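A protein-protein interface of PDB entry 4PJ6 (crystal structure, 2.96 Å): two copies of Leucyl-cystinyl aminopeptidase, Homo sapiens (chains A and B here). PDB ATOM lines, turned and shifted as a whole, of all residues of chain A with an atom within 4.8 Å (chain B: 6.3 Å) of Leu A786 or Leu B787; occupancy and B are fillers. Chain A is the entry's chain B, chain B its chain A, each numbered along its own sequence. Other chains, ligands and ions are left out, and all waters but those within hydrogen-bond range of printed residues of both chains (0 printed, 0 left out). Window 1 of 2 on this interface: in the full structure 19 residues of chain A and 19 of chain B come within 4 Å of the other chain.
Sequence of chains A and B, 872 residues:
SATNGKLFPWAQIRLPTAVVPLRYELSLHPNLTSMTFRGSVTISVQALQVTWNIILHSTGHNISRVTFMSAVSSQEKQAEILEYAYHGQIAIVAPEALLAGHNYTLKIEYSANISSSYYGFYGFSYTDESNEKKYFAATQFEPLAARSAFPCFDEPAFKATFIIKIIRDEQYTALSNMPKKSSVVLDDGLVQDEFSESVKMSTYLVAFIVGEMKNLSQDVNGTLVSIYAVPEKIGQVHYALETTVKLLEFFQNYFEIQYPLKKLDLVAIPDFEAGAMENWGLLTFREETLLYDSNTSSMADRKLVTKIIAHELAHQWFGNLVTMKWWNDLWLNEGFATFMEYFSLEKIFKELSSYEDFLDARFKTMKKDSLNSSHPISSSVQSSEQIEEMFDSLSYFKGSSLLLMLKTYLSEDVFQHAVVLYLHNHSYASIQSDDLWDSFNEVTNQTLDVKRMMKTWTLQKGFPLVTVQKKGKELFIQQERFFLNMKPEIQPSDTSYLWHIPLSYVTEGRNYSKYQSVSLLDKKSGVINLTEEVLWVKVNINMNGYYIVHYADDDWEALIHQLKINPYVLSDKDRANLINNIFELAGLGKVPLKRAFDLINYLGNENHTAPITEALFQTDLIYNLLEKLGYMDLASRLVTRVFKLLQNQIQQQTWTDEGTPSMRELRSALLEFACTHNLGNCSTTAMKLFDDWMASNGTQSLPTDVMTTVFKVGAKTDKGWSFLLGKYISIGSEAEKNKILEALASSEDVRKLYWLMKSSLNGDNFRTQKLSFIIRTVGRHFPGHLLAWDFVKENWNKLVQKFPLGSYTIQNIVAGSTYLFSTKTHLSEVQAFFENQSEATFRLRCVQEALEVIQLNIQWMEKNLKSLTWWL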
ATOM      1  N   PHE A 782     -14.380  14.641  -7.217  1.00  0.00           N
ATOM      2  CA  PHE A 782     -13.942  15.990  -7.427  1.00  0.00           C
ATOM      3  C   PHE A 782     -12.465  16.135  -7.754  1.00  0.00           C
ATOM      4  O   PHE A 782     -12.137  16.878  -8.675  1.00  0.00           O
ATOM      5  CB  PHE A 782     -14.373  16.935  -6.314  1.00  0.00           C
ATOM      6  CG  PHE A 782     -14.392  18.382  -6.736  1.00  0.00           C
ATOM      7  CD1 PHE A 782     -15.426  18.881  -7.534  1.00  0.00           C
ATOM      8  CD2 PHE A 782     -13.375  19.240  -6.343  1.00  0.00           C
ATOM      9  CE1 PHE A 782     -15.437  20.206  -7.911  1.00  0.00           C
ATOM     10  CE2 PHE A 782     -13.383  20.566  -6.725  1.00  0.00           C
ATOM     11  CZ  PHE A 782     -14.417  21.047  -7.501  1.00  0.00           C
ATOM     12  N   GLY A 784     -10.417  14.267  -9.281  1.00  0.00           N
ATOM     13  CA  GLY A 784     -10.069  13.690 -10.566  1.00  0.00           C
ATOM     14  C   GLY A 784     -10.995  14.045 -11.705  1.00  0.00           C
ATOM     15  O   GLY A 784     -10.813  13.571 -12.832  1.00  0.00           O
ATOM     16  N   HIS A 785     -11.993  14.874 -11.445  1.00  0.00           N
ATOM     17  CA  HIS A 785     -12.918  15.206 -12.510  1.00  0.00           C
ATOM     18  C   HIS A 785     -12.202  15.881 -13.724  1.00  0.00           C
ATOM     19  O   HIS A 785     -12.242  15.358 -14.839  1.00  0.00           O
ATOM     20  CB  HIS A 785     -14.085  16.037 -11.996  1.00  0.00           C
ATOM     21  CG  HIS A 785     -15.120  16.284 -13.039  1.00  0.00           C
ATOM     22  ND1 HIS A 785     -15.646  17.531 -13.293  1.00  0.00           N
ATOM     23  CD2 HIS A 785     -15.684  15.441 -13.936  1.00  0.00           C
ATOM     24  CE1 HIS A 785     -16.498  17.444 -14.301  1.00  0.00           C
ATOM     25  NE2 HIS A 785     -16.546  16.186 -14.707  1.00  0.00           N
ATOM     26  N   LEU A 786     -11.526  17.013 -13.518  1.00  0.00           N
ATOM     27  CA  LEU A 786     -10.826  17.654 -14.652  1.00  0.00           C
ATOM     28  C   LEU A 786      -9.666  16.777 -15.118  1.00  0.00           C
ATOM     29  O   LEU A 786      -9.281  16.841 -16.287  1.00  0.00           O
ATOM     30  CB  LEU A 786     -10.361  19.081 -14.337  1.00  0.00           C
ATOM     31  CG  LEU A 786     -11.491  19.995 -13.906  1.00  0.00           C
ATOM     32  CD1 LEU A 786     -10.996  21.136 -13.039  1.00  0.00           C
ATOM     33  CD2 LEU A 786     -12.215  20.513 -15.137  1.00  0.00           C
ATOM     34  N   LEU A 787      -9.138  15.942 -14.213  1.00  0.00           N
ATOM     35  CA  LEU A 787      -7.950  15.153 -14.500  1.00  0.00           C
ATOM     36  C   LEU A 787      -8.279  13.996 -15.383  1.00  0.00           C
ATOM     37  O   LEU A 787      -7.457  13.617 -16.204  1.00  0.00           O
ATOM     38  CB  LEU A 787      -7.258  14.654 -13.225  1.00  0.00           C
ATOM     39  CG  LEU A 787      -5.889  13.973 -13.385  1.00  0.00           C
ATOM     40  CD1 LEU A 787      -4.799  14.993 -13.581  1.00  0.00           C
ATOM     41  CD2 LEU A 787      -5.589  13.166 -12.156  1.00  0.00           C
ATOM     42  N   ALA A 788      -9.460  13.421 -15.237  1.00  0.00           N
ATOM     43  CA  ALA A 788      -9.755  12.291 -16.070  1.00  0.00           C
ATOM     44  C   ALA A 788      -9.931  12.714 -17.534  1.00  0.00           C
ATOM     45  O   ALA A 788      -9.278  12.157 -18.413  1.00  0.00           O
ATOM     46  CB  ALA A 788     -10.965  11.563 -15.551  1.00  0.00           C
ATOM     47  N   TRP A 789     -10.756  13.732 -17.784  1.00  0.00           N
ATOM     48  CA  TRP A 789     -11.006  14.219 -19.118  1.00  0.00           C
ATOM     49  C   TRP A 789      -9.721  14.733 -19.736  1.00  0.00           C
ATOM     50  O   TRP A 789      -9.487  14.513 -20.927  1.00  0.00           O
ATOM     51  CB  TRP A 789     -12.154  15.280 -19.112  1.00  0.00           C
ATOM     52  CG  TRP A 789     -12.373  16.072 -20.410  1.00  0.00           C
ATOM     53  CD1 TRP A 789     -12.350  17.437 -20.552  1.00  0.00           C
ATOM     54  CD2 TRP A 789     -12.612  15.534 -21.715  1.00  0.00           C
ATOM     55  NE1 TRP A 789     -12.557  17.781 -21.874  1.00  0.00           N
ATOM     56  CE2 TRP A 789     -12.723  16.640 -22.610  1.00  0.00           C
ATOM     57  CE3 TRP A 789     -12.715  14.229 -22.221  1.00  0.00           C
ATOM     58  CZ2 TRP A 789     -12.936  16.483 -23.978  1.00  0.00           C
ATOM     59  CZ3 TRP A 789     -12.921  14.061 -23.585  1.00  0.00           C
ATOM     60  CH2 TRP A 789     -13.029  15.190 -24.453  1.00  0.00           C
ATOM     61  N   ASP A 790      -8.891  15.412 -18.941  1.00  0.00           N
ATOM     62  CA  ASP A 790      -7.618  15.958 -19.470  1.00  0.00           C
ATOM     63  C   ASP A 790      -6.761  14.830 -20.045  1.00  0.00           C
ATOM     64  O   ASP A 790      -6.256  14.940 -21.163  1.00  0.00           O
ATOM     65  CB  ASP A 790      -6.861  16.747 -18.414  1.00  0.00           C
ATOM     66  CG  ASP A 790      -5.611  17.387 -18.955  1.00  0.00           C
ATOM     67  OD1 ASP A 790      -5.686  18.524 -19.459  1.00  0.00           O
ATOM     68  OD2 ASP A 790      -4.535  16.760 -18.882  1.00  0.00           O
ATOM     69  N   PHE A 821     -20.061  17.050 -17.129  1.00  0.00           N
ATOM     70  CA  PHE A 821     -19.856  18.425 -17.579  1.00  0.00           C
ATOM     71  C   PHE A 821     -21.237  18.999 -17.813  1.00  0.00           C
ATOM     72  O   PHE A 821     -21.986  18.459 -18.625  1.00  0.00           O
ATOM     73  CB  PHE A 821     -19.051  18.458 -18.875  1.00  0.00           C
ATOM     74  CG  PHE A 821     -17.574  18.200 -18.706  1.00  0.00           C
ATOM     75  CD1 PHE A 821     -16.862  18.668 -17.572  1.00  0.00           C
ATOM     76  CD2 PHE A 821     -16.863  17.523 -19.710  1.00  0.00           C
ATOM     77  CE1 PHE A 821     -15.485  18.429 -17.441  1.00  0.00           C
ATOM     78  CE2 PHE A 821     -15.495  17.284 -19.581  1.00  0.00           C
ATOM     79  CZ  PHE A 821     -14.803  17.735 -18.447  1.00  0.00           C
ATOM     80  N   HIS A 826     -17.952  24.055 -20.957  1.00  0.00           N
ATOM     81  CA  HIS A 826     -17.447  22.724 -21.111  1.00  0.00           C
ATOM     82  C   HIS A 826     -17.895  22.173 -22.460  1.00  0.00           C
ATOM     83  O   HIS A 826     -17.073  21.619 -23.212  1.00  0.00           O
ATOM     84  CB  HIS A 826     -17.875  21.849 -19.938  1.00  0.00           C
ATOM     85  CG  HIS A 826     -16.955  21.949 -18.762  1.00  0.00           C
ATOM     86  ND1 HIS A 826     -15.624  21.588 -18.829  1.00  0.00           N
ATOM     87  CD2 HIS A 826     -17.163  22.379 -17.493  1.00  0.00           C
ATOM     88  CE1 HIS A 826     -15.056  21.793 -17.652  1.00  0.00           C
ATOM     89  NE2 HIS A 826     -15.966  22.277 -16.825  1.00  0.00           N
ATOM     90  N   ASP B 749      -5.529  19.523  -1.258  1.00  0.00           N
ATOM     91  CA  ASP B 749      -6.973  19.210  -1.213  1.00  0.00           C
ATOM     92  C   ASP B 749      -7.676  20.061  -2.279  1.00  0.00           C
ATOM     93  O   ASP B 749      -7.981  21.254  -2.095  1.00  0.00           O
ATOM     94  CB  ASP B 749      -7.564  19.494   0.181  1.00  0.00           C
ATOM     95  CG  ASP B 749      -8.891  18.751   0.449  1.00  0.00           C
ATOM     96  OD1 ASP B 749      -9.690  18.507  -0.484  1.00  0.00           O
ATOM     97  OD2 ASP B 749      -9.133  18.406   1.625  1.00  0.00           O
ATOM     98  N   VAL B 750      -7.876  19.439  -3.419  1.00  0.00           N
ATOM     99  CA  VAL B 750      -8.437  20.110  -4.553  1.00  0.00           C
ATOM    100  C   VAL B 750      -9.691  20.907  -4.153  1.00  0.00           C
ATOM    101  O   VAL B 750      -9.911  22.040  -4.669  1.00  0.00           O
ATOM    102  CB  VAL B 750      -8.696  19.079  -5.652  1.00  0.00           C
ATOM    103  CG1 VAL B 750      -9.503  19.682  -6.786  1.00  0.00           C
ATOM    104  CG2 VAL B 750      -7.364  18.539  -6.136  1.00  0.00           C
ATOM    105  N   ARG B 751     -10.476  20.326  -3.221  1.00  0.00           N
ATOM    106  CA  ARG B 751     -11.735  20.922  -2.746  1.00  0.00           C
ATOM    107  C   ARG B 751     -11.451  22.178  -2.001  1.00  0.00           C
ATOM    108  O   ARG B 751     -12.104  23.192  -2.212  1.00  0.00           O
ATOM    109  CB  ARG B 751     -12.516  19.976  -1.850  1.00  0.00           C
ATOM    110  CG  ARG B 751     -13.479  19.063  -2.589  1.00  0.00           C
ATOM    111  CD  ARG B 751     -13.927  17.928  -1.676  1.00  0.00           C
ATOM    112  NE  ARG B 751     -13.580  16.644  -2.286  1.00  0.00           N
ATOM    113  CZ  ARG B 751     -14.446  15.805  -2.831  1.00  0.00           C
ATOM    114  NH1 ARG B 751     -15.742  16.075  -2.815  1.00  0.00           N
ATOM    115  NH2 ARG B 751     -14.001  14.693  -3.384  1.00  0.00           N
ATOM    116  N   LEU B 753      -8.868  24.053  -2.332  1.00  0.00           N
ATOM    117  CA  LEU B 753      -8.386  25.036  -3.308  1.00  0.00           C
ATOM    118  C   LEU B 753      -9.538  25.707  -4.011  1.00  0.00           C
ATOM    119  O   LEU B 753      -9.583  26.930  -4.083  1.00  0.00           O
ATOM    120  CB  LEU B 753      -7.443  24.417  -4.346  1.00  0.00           C
ATOM    121  CG  LEU B 753      -6.153  23.862  -3.773  1.00  0.00           C
ATOM    122  CD1 LEU B 753      -5.426  23.040  -4.822  1.00  0.00           C
ATOM    123  CD2 LEU B 753      -5.288  25.005  -3.254  1.00  0.00           C
ATOM    124  N   TYR B 754     -10.471  24.898  -4.500  1.00  0.00           N
ATOM    125  CA  TYR B 754     -11.645  25.411  -5.160  1.00  0.00           C
ATOM    126  C   TYR B 754     -12.312  26.431  -4.285  1.00  0.00           C
ATOM    127  O   TYR B 754     -12.536  27.554  -4.732  1.00  0.00           O
ATOM    128  CB  TYR B 754     -12.637  24.307  -5.480  1.00  0.00           C
ATOM    129  CG  TYR B 754     -13.904  24.855  -6.116  1.00  0.00           C
ATOM    130  CD1 TYR B 754     -13.895  25.384  -7.412  1.00  0.00           C
ATOM    131  CD2 TYR B 754     -15.104  24.847  -5.428  1.00  0.00           C
ATOM    132  CE1 TYR B 754     -15.040  25.905  -7.985  1.00  0.00           C
ATOM    133  CE2 TYR B 754     -16.253  25.369  -6.006  1.00  0.00           C
ATOM    134  CZ  TYR B 754     -16.210  25.896  -7.288  1.00  0.00           C
ATOM    135  OH  TYR B 754     -17.347  26.408  -7.882  1.00  0.00           O
ATOM    136  N   MET B 757     -10.874  29.774  -3.985  1.00  0.00           N
ATOM    137  CA  MET B 757     -11.062  30.658  -5.158  1.00  0.00           C
ATOM    138  C   MET B 757     -12.452  31.195  -5.148  1.00  0.00           C
ATOM    139  O   MET B 757     -12.604  32.400  -5.122  1.00  0.00           O
ATOM    140  CB  MET B 757     -10.682  30.015  -6.496  1.00  0.00           C
ATOM    141  CG  MET B 757      -9.195  29.761  -6.608  1.00  0.00           C
ATOM    142  SD  MET B 757      -8.830  28.780  -8.033  1.00  0.00           S
ATOM    143  CE  MET B 757      -9.472  27.153  -7.675  1.00  0.00           C
ATOM    144  N   VAL B 778      -2.691  28.424  -6.651  1.00  0.00           N
ATOM    145  CA  VAL B 778      -3.340  27.153  -6.906  1.00  0.00           C
ATOM    146  C   VAL B 778      -2.788  26.549  -8.188  1.00  0.00           C
ATOM    147  O   VAL B 778      -2.359  25.404  -8.197  1.00  0.00           O
ATOM    148  CB  VAL B 778      -4.877  27.304  -6.986  1.00  0.00           C
ATOM    149  CG1 VAL B 778      -5.555  25.995  -7.440  1.00  0.00           C
ATOM    150  CG2 VAL B 778      -5.467  27.772  -5.666  1.00  0.00           C
ATOM    151  N   PRO B 783      -2.011  19.492  -7.868  1.00  0.00           N
ATOM    152  CA  PRO B 783      -3.433  19.266  -7.645  1.00  0.00           C
ATOM    153  C   PRO B 783      -4.307  20.426  -8.080  1.00  0.00           C
ATOM    154  O   PRO B 783      -5.476  20.256  -8.363  1.00  0.00           O
ATOM    155  CB  PRO B 783      -3.499  19.066  -6.131  1.00  0.00           C
ATOM    156  CG  PRO B 783      -2.154  18.559  -5.779  1.00  0.00           C
ATOM    157  CD  PRO B 783      -1.267  19.433  -6.599  1.00  0.00           C
ATOM    158  N   GLY B 784      -3.772  21.620  -8.136  1.00  0.00           N
ATOM    159  CA  GLY B 784      -4.634  22.690  -8.654  1.00  0.00           C
ATOM    160  C   GLY B 784      -4.353  23.249 -10.051  1.00  0.00           C
ATOM    161  O   GLY B 784      -4.700  24.387 -10.337  1.00  0.00           O
ATOM    162  N   HIS B 785      -3.665  22.506 -10.896  1.00  0.00           N
ATOM    163  CA  HIS B 785      -3.157  23.101 -12.127  1.00  0.00           C
ATOM    164  C   HIS B 785      -4.361  23.338 -13.095  1.00  0.00           C
ATOM    165  O   HIS B 785      -4.574  24.458 -13.578  1.00  0.00           O
ATOM    166  CB  HIS B 785      -2.002  22.248 -12.759  1.00  0.00           C
ATOM    167  CG  HIS B 785      -1.606  22.690 -14.127  1.00  0.00           C
ATOM    168  ND1 HIS B 785      -1.131  23.962 -14.374  1.00  0.00           N
ATOM    169  CD2 HIS B 785      -1.644  22.061 -15.333  1.00  0.00           C
ATOM    170  CE1 HIS B 785      -0.894  24.102 -15.676  1.00  0.00           C
ATOM    171  NE2 HIS B 785      -1.188  22.957 -16.279  1.00  0.00           N
ATOM    172  N   LEU B 786      -5.104  22.257 -13.387  1.00  0.00           N
ATOM    173  CA  LEU B 786      -6.226  22.301 -14.307  1.00  0.00           C
ATOM    174  C   LEU B 786      -7.405  23.087 -13.682  1.00  0.00           C
ATOM    175  O   LEU B 786      -8.142  23.798 -14.406  1.00  0.00           O
ATOM    176  CB  LEU B 786      -6.679  20.887 -14.612  1.00  0.00           C
ATOM    177  CG  LEU B 786      -5.750  19.940 -15.359  1.00  0.00           C
ATOM    178  CD1 LEU B 786      -6.402  18.573 -15.395  1.00  0.00           C
ATOM    179  CD2 LEU B 786      -5.470  20.374 -16.786  1.00  0.00           C
ATOM    180  N   LEU B 787      -7.557  22.935 -12.351  1.00  0.00           N
ATOM    181  CA  LEU B 787      -8.583  23.582 -11.515  1.00  0.00           C
ATOM    182  C   LEU B 787      -8.584  25.072 -11.673  1.00  0.00           C
ATOM    183  O   LEU B 787      -9.619  25.655 -11.962  1.00  0.00           O
ATOM    184  CB  LEU B 787      -8.341  23.248 -10.039  1.00  0.00           C
ATOM    185  CG  LEU B 787      -9.449  23.521  -9.034  1.00  0.00           C
ATOM    186  CD1 LEU B 787     -10.464  22.401  -9.101  1.00  0.00           C
ATOM    187  CD2 LEU B 787      -8.869  23.551  -7.637  1.00  0.00           C
ATOM    188  N   ALA B 788      -7.405  25.665 -11.470  1.00  0.00           N
ATOM    189  CA  ALA B 788      -7.195  27.118 -11.532  1.00  0.00           C
ATOM    190  C   ALA B 788      -7.632  27.711 -12.900  1.00  0.00           C
ATOM    191  O   ALA B 788      -8.265  28.736 -12.946  1.00  0.00           O
ATOM    192  CB  ALA B 788      -5.724  27.446 -11.226  1.00  0.00           C
ATOM    193  N   TRP B 789      -7.268  27.040 -13.990  1.00  0.00           N
ATOM    194  CA  TRP B 789      -7.567  27.475 -15.340  1.00  0.00           C
ATOM    195  C   TRP B 789      -9.064  27.305 -15.668  1.00  0.00           C
ATOM    196  O   TRP B 789      -9.646  28.156 -16.340  1.00  0.00           O
ATOM    197  CB  TRP B 789      -6.661  26.772 -16.398  1.00  0.00           C
ATOM    198  CG  TRP B 789      -7.097  27.035 -17.876  1.00  0.00           C
ATOM    199  CD1 TRP B 789      -7.390  26.102 -18.808  1.00  0.00           C
ATOM    200  CD2 TRP B 789      -7.302  28.304 -18.499  1.00  0.00           C
ATOM    201  NE1 TRP B 789      -7.753  26.692 -19.975  1.00  0.00           N
ATOM    202  CE2 TRP B 789      -7.708  28.050 -19.825  1.00  0.00           C
ATOM    203  CE3 TRP B 789      -7.163  29.626 -18.078  1.00  0.00           C
ATOM    204  CZ2 TRP B 789      -7.993  29.077 -20.751  1.00  0.00           C
ATOM    205  CZ3 TRP B 789      -7.442  30.656 -18.998  1.00  0.00           C
ATOM    206  CH2 TRP B 789      -7.861  30.372 -20.315  1.00  0.00           C
ATOM    207  N   ASP B 790      -9.662  26.213 -15.189  1.00  0.00           N
ATOM    208  CA  ASP B 790     -11.118  25.965 -15.291  1.00  0.00           C
ATOM    209  C   ASP B 790     -11.891  27.053 -14.532  1.00  0.00           C
ATOM    210  O   ASP B 790     -12.905  27.537 -15.006  1.00  0.00           O
ATOM    211  CB  ASP B 790     -11.445  24.570 -14.721  1.00  0.00           C
ATOM    212  CG  ASP B 790     -12.858  24.136 -14.979  1.00  0.00           C
ATOM    213  OD1 ASP B 790     -13.203  23.855 -16.148  1.00  0.00           O
ATOM    214  OD2 ASP B 790     -13.618  24.030 -13.987  1.00  0.00           O
ATOM    215  N   PHE B 791     -11.402  27.437 -13.352  1.00  0.00           N
ATOM    216  CA  PHE B 791     -12.078  28.452 -12.534  1.00  0.00           C
ATOM    217  C   PHE B 791     -12.081  29.768 -13.317  1.00  0.00           C
ATOM    218  O   PHE B 791     -13.123  30.410 -13.449  1.00  0.00           O
ATOM    219  CB  PHE B 791     -11.416  28.601 -11.136  1.00  0.00           C
ATOM    220  CG  PHE B 791     -12.142  29.546 -10.231  1.00  0.00           C
ATOM    221  CD1 PHE B 791     -13.231  29.117  -9.513  1.00  0.00           C
ATOM    222  CD2 PHE B 791     -11.749  30.863 -10.124  1.00  0.00           C
ATOM    223  CE1 PHE B 791     -13.905  29.981  -8.683  1.00  0.00           C
ATOM    224  CE2 PHE B 791     -12.422  31.744  -9.312  1.00  0.00           C
ATOM    225  CZ  PHE B 791     -13.504  31.301  -8.585  1.00  0.00           C
ATOM    226  N   VAL B 792     -10.913  30.136 -13.838  1.00  0.00           N
ATOM    227  CA  VAL B 792     -10.751  31.310 -14.680  1.00  0.00           C
ATOM    228  C   VAL B 792     -11.784  31.291 -15.845  1.00  0.00           C
ATOM    229  O   VAL B 792     -12.511  32.259 -16.052  1.00  0.00           O
ATOM    230  CB  VAL B 792      -9.294  31.418 -15.186  1.00  0.00           C
ATOM    231  CG1 VAL B 792      -9.160  32.481 -16.265  1.00  0.00           C
ATOM    232  CG2 VAL B 792      -8.370  31.736 -14.030  1.00  0.00           C
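The side-chain carboxylate (OD1) of Asp B790 lies close to a ring nitrogen (NE2) of His A826, at 3.3 Å.
The side-chain carboxylate (OD1) of Asp B749 lies close to the backbone NH (N) of Arg B751, at 3.4 Å.
CD2 of Phe A782 touches CG1 of Val B750, at 3.9 Å. Phe A782 touches Arg B751 (CB to CZ, 3.7 Å). Leu A786 touches Leu B786 (O to CD1, 3.5 Å). Leu A786 touches Leu B787. Leu A786 touches Asp B790 (CD2 to OD1, 3.6 Å). CD1 of Leu B786 touches CA of Leu A787, 3.9 Å away. Asp A790 touches Leu B786 (OD1 to CD2, 3.3 Å).
Of the printed residues of chain B, Phe A782 touches Val B750 and Arg B751. Of chain B, only Leu B786, Leu B787 and Asp B790 come within 4 Å of Leu A786. Of the printed residues of chain B, Leu A787 touches Leu B786 (3.9 Å). Printed residues of chain B within 4 Å of Asp A790: Leu B786. Of the printed residues of chain B, His A826 touches Asp B790 (3.2 Å). Printed residues of chain A within 4 Å of Arg B751: Phe A782. The nearest residue of chain B that does not touch Leu A786 is Ala B788 (6.0 Å).
Hydrophobic or aromatic side chains of chain A within 4 Å of the printed part of chain B: Phe A782, Leu A786 and His A826. Hydrophobic or aromatic side chains of chain B within 4 Å of the printed part of chain A: Val B750 and Leu B786.
Leu B786 touches its own counterpart, Leu A786. Leu A786 touches Leu B787, and with the chains exchanged Leu A787 touches Leu B786. Leu A786 touches Asp B790, and with the chains exchanged Asp A790 touches Leu B786. Positions printed for both chains: 784, 785, 786, 787, 788, 789 and 790.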
